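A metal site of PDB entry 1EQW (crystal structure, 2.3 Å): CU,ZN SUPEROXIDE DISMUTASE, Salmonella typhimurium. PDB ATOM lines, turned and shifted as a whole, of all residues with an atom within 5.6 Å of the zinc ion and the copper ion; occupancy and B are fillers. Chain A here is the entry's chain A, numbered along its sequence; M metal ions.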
ATOM      1  N   PHE A  47      23.081 -10.729  10.261  1.00  0.00           N
ATOM      2  CA  PHE A  47      22.260 -10.015   9.279  1.00  0.00           C
ATOM      3  C   PHE A  47      21.731 -11.019   8.246  1.00  0.00           C
ATOM      4  O   PHE A  47      22.499 -11.506   7.420  1.00  0.00           O
ATOM      5  CB  PHE A  47      23.121  -8.941   8.600  1.00  0.00           C
ATOM      6  CG  PHE A  47      22.473  -8.117   7.528  1.00  0.00           C
ATOM      7  CD1 PHE A  47      21.206  -7.562   7.711  1.00  0.00           C
ATOM      8  CD2 PHE A  47      23.134  -7.896   6.331  1.00  0.00           C
ATOM      9  CE1 PHE A  47      20.619  -6.794   6.709  1.00  0.00           C
ATOM     10  CE2 PHE A  47      22.560  -7.123   5.314  1.00  0.00           C
ATOM     11  CZ  PHE A  47      21.300  -6.575   5.500  1.00  0.00           C
ATOM     12  N   HIS A  48      20.429 -11.302   8.285  1.00  0.00           N
ATOM     13  CA  HIS A  48      19.858 -12.283   7.360  1.00  0.00           C
ATOM     14  C   HIS A  48      18.496 -11.899   6.801  1.00  0.00           C
ATOM     15  O   HIS A  48      17.788 -11.065   7.365  1.00  0.00           O
ATOM     16  CB  HIS A  48      19.709 -13.654   7.997  1.00  0.00           C
ATOM     17  CG  HIS A  48      20.691 -13.894   9.145  1.00  0.00           C
ATOM     18  ND1 HIS A  48      20.344 -13.844  10.471  1.00  0.00           N
ATOM     19  CD2 HIS A  48      22.010 -14.192   9.102  1.00  0.00           C
ATOM     20  CE1 HIS A  48      21.400 -14.107  11.208  1.00  0.00           C
ATOM     21  NE2 HIS A  48      22.432 -14.317  10.406  1.00  0.00           N
ATOM     22  N   HIS A  50      14.790 -12.973   6.237  1.00  0.00           N
ATOM     23  CA  HIS A  50      13.843 -13.915   6.810  1.00  0.00           C
ATOM     24  C   HIS A  50      12.631 -14.148   5.879  1.00  0.00           C
ATOM     25  O   HIS A  50      12.252 -13.298   5.070  1.00  0.00           O
ATOM     26  CB  HIS A  50      13.416 -13.442   8.184  1.00  0.00           C
ATOM     27  CG  HIS A  50      14.491 -13.692   9.271  1.00  0.00           C
ATOM     28  ND1 HIS A  50      14.244 -14.330  10.467  1.00  0.00           N
ATOM     29  CD2 HIS A  50      15.810 -13.353   9.291  1.00  0.00           C
ATOM     30  CE1 HIS A  50      15.360 -14.373  11.177  1.00  0.00           C
ATOM     31  NE2 HIS A  50      16.324 -13.786  10.489  1.00  0.00           N
ATOM     32  N   HIS A  73      15.078 -18.052   8.873  1.00  0.00           N
ATOM     33  CA  HIS A  73      15.937 -17.591   7.795  1.00  0.00           C
ATOM     34  C   HIS A  73      15.473 -18.144   6.459  1.00  0.00           C
ATOM     35  O   HIS A  73      15.143 -19.329   6.362  1.00  0.00           O
ATOM     36  CB  HIS A  73      17.367 -18.062   8.008  1.00  0.00           C
ATOM     37  CG  HIS A  73      18.039 -17.355   9.177  1.00  0.00           C
ATOM     38  ND1 HIS A  73      19.392 -17.474   9.432  1.00  0.00           N
ATOM     39  CD2 HIS A  73      17.543 -16.547  10.142  1.00  0.00           C
ATOM     40  CE1 HIS A  73      19.698 -16.768  10.505  1.00  0.00           C
ATOM     41  NE2 HIS A  73      18.596 -16.199  10.957  1.00  0.00           N
ATOM     42  N   LYS A  81      20.487 -25.654   7.531  1.00  0.00           N
ATOM     43  CA  LYS A  81      21.842 -25.343   7.968  1.00  0.00           C
ATOM     44  C   LYS A  81      22.242 -23.901   7.675  1.00  0.00           C
ATOM     45  O   LYS A  81      22.125 -23.421   6.546  1.00  0.00           O
ATOM     46  CB  LYS A  81      22.829 -26.309   7.293  1.00  0.00           C
ATOM     47  CG  LYS A  81      22.534 -27.775   7.569  1.00  0.00           C
ATOM     48  CD  LYS A  81      23.592 -28.700   6.965  1.00  0.00           C
ATOM     49  CE  LYS A  81      23.358 -30.143   7.391  1.00  0.00           C
ATOM     50  NZ  LYS A  81      24.367 -31.064   6.802  1.00  0.00           N
ATOM     51  N   HIS A  82      22.735 -23.223   8.704  1.00  0.00           N
ATOM     52  CA  HIS A  82      23.190 -21.862   8.601  1.00  0.00           C
ATOM     53  C   HIS A  82      24.670 -21.837   8.316  1.00  0.00           C
ATOM     54  O   HIS A  82      25.497 -21.927   9.216  1.00  0.00           O
ATOM     55  CB  HIS A  82      22.837 -21.130   9.907  1.00  0.00           C
ATOM     56  CG  HIS A  82      23.275 -19.658   9.894  1.00  0.00           C
ATOM     57  ND1 HIS A  82      22.614 -18.704   9.144  1.00  0.00           N
ATOM     58  CD2 HIS A  82      24.278 -19.017  10.525  1.00  0.00           C
ATOM     59  CE1 HIS A  82      23.208 -17.533   9.330  1.00  0.00           C
ATOM     60  NE2 HIS A  82      24.215 -17.699  10.164  1.00  0.00           N
ATOM     61  N   LEU A  83      25.051 -21.683   7.017  1.00  0.00           N
ATOM     62  CA  LEU A  83      26.475 -21.779   6.675  1.00  0.00           C
ATOM     63  C   LEU A  83      27.028 -20.425   6.212  1.00  0.00           C
ATOM     64  O   LEU A  83      28.245 -20.372   5.870  1.00  0.00           O
ATOM     65  CB  LEU A  83      26.692 -22.823   5.581  1.00  0.00           C
ATOM     66  CG  LEU A  83      26.278 -24.262   5.916  1.00  0.00           C
ATOM     67  CD1 LEU A  83      26.550 -25.191   4.731  1.00  0.00           C
ATOM     68  CD2 LEU A  83      26.996 -24.758   7.152  1.00  0.00           C
ATOM     69  N   HIS A  91      21.337 -21.621   4.369  1.00  0.00           N
ATOM     70  CA  HIS A  91      20.257 -20.657   4.187  1.00  0.00           C
ATOM     71  C   HIS A  91      20.519 -19.647   3.112  1.00  0.00           C
ATOM     72  O   HIS A  91      21.459 -18.860   3.225  1.00  0.00           O
ATOM     73  CB  HIS A  91      20.045 -19.890   5.499  1.00  0.00           C
ATOM     74  CG  HIS A  91      19.680 -20.772   6.692  1.00  0.00           C
ATOM     75  ND1 HIS A  91      20.211 -20.565   7.954  1.00  0.00           N
ATOM     76  CD2 HIS A  91      18.844 -21.828   6.799  1.00  0.00           C
ATOM     77  CE1 HIS A  91      19.712 -21.460   8.783  1.00  0.00           C
ATOM     78  NE2 HIS A  91      18.884 -22.241   8.113  1.00  0.00           N
ATOM     79  N   GLY A  93      19.140 -17.080   2.605  1.00  0.00           N
ATOM     80  CA  GLY A  93      18.975 -15.773   3.231  1.00  0.00           C
ATOM     81  C   GLY A  93      20.157 -15.311   4.055  1.00  0.00           C
ATOM     82  O   GLY A  93      20.132 -14.218   4.617  1.00  0.00           O
ATOM     83  N   ASP A  94      21.206 -16.129   4.141  1.00  0.00           N
ATOM     84  CA  ASP A  94      22.376 -15.775   4.945  1.00  0.00           C
ATOM     85  C   ASP A  94      23.233 -14.693   4.293  1.00  0.00           C
ATOM     86  O   ASP A  94      23.897 -14.925   3.282  1.00  0.00           O
ATOM     87  CB  ASP A  94      23.233 -17.022   5.200  1.00  0.00           C
ATOM     88  CG  ASP A  94      22.610 -17.966   6.217  1.00  0.00           C
ATOM     89  OD1 ASP A  94      21.535 -17.637   6.758  1.00  0.00           O
ATOM     90  OD2 ASP A  94      23.194 -19.032   6.485  1.00  0.00           O
ATOM     91  N   MET A 127      16.743  -8.855   8.586  1.00  0.00           N
ATOM     92  CA  MET A 127      16.878  -8.886  10.034  1.00  0.00           C
ATOM     93  C   MET A 127      18.280  -8.578  10.561  1.00  0.00           C
ATOM     94  O   MET A 127      19.284  -9.006   9.983  1.00  0.00           O
ATOM     95  CB  MET A 127      16.470 -10.266  10.553  1.00  0.00           C
ATOM     96  CG  MET A 127      16.063 -10.283  12.021  1.00  0.00           C
ATOM     97  SD  MET A 127      14.312  -9.932  12.264  1.00  0.00           S
ATOM     98  CE  MET A 127      14.235  -9.801  14.046  1.00  0.00           C
ATOM     99  N   HIS A 129      20.268  -8.950  14.103  1.00  0.00           N
ATOM    100  CA  HIS A 129      20.227  -9.548  15.437  1.00  0.00           C
ATOM    101  C   HIS A 129      21.113  -8.816  16.429  1.00  0.00           C
ATOM    102  O   HIS A 129      21.885  -7.941  16.051  1.00  0.00           O
ATOM    103  CB  HIS A 129      20.679 -10.989  15.369  1.00  0.00           C
ATOM    104  CG  HIS A 129      19.781 -11.870  14.491  1.00  0.00           C
ATOM    105  ND1 HIS A 129      18.858 -12.739  15.014  1.00  0.00           N
ATOM    106  CD2 HIS A 129      19.680 -11.964  13.148  1.00  0.00           C
ATOM    107  CE1 HIS A 129      18.222 -13.346  14.026  1.00  0.00           C
ATOM    108  NE2 HIS A 129      18.703 -12.900  12.877  1.00  0.00           N
ATOM    109  N   LEU A 142      22.540 -20.911  14.440  1.00  0.00           N
ATOM    110  CA  LEU A 142      22.319 -19.699  13.653  1.00  0.00           C
ATOM    111  C   LEU A 142      23.386 -18.628  13.868  1.00  0.00           C
ATOM    112  O   LEU A 142      23.091 -17.458  14.133  1.00  0.00           O
ATOM    113  CB  LEU A 142      20.926 -19.123  13.993  1.00  0.00           C
ATOM    114  CG  LEU A 142      19.700 -19.718  13.290  1.00  0.00           C
ATOM    115  CD1 LEU A 142      19.968 -21.154  12.876  1.00  0.00           C
ATOM    116  CD2 LEU A 142      18.486 -19.627  14.183  1.00  0.00           C
HETATM  117 ZN    ZN M   1      20.838 -18.672   8.455  1.00  0.00          ZN
HETATM  118 CU    CU M   2      18.195 -13.781  11.253  1.00  0.00          CU
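Four residues have an atom within 4 Å of the zinc ion: His 73, His 82, His 91 and Asp 94.
The nearest printed residue that does not touch the zinc ion is His 48 (4.7 Å).
Met 127 touches the copper ion (CB to CU, 3.98 Å).
Of the 13 residues printed, 5 come within 4 Å of the copper ion.
The nearest printed residue that does not touch the copper ion is Phe 47 (5.4 Å).
The zinc ion is bound by a ring nitrogen (ND1) of His 82 (1.9 Å), a ring nitrogen (ND1) of His 91 (2.1 Å), the side-chain carboxylate of Asp 94 (2.1 Å) and a ring nitrogen (ND1) of His 73 (2.1 Å).
The zinc ion has four donor atoms within binding distance.
The backbone NH (N) of His 91 is in hydrogen-bond range of the backbone carbonyl oxygen (O) of Lys 81 (2.9 Å).
The side-chain carboxylate (OD2) of Asp 94 lies within hydrogen-bond range of the backbone NH (N) of Leu 83 (3.3 Å).
The backbone NH of Met 127 is in hydrogen-bond range of the backbone carbonyl oxygen of His 48 (2.7 Å).
A ring nitrogen (NE2) of His 129 is bound to the copper ion (1.9 Å).
NE2 of His 50 binds the copper ion, at 2.0 Å.
The copper ion is bound by ND1 of His 48, at 2.3 Å.
NE2 of His 73 is bound to the copper ion.
The copper ion has four donor atoms within binding distance.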
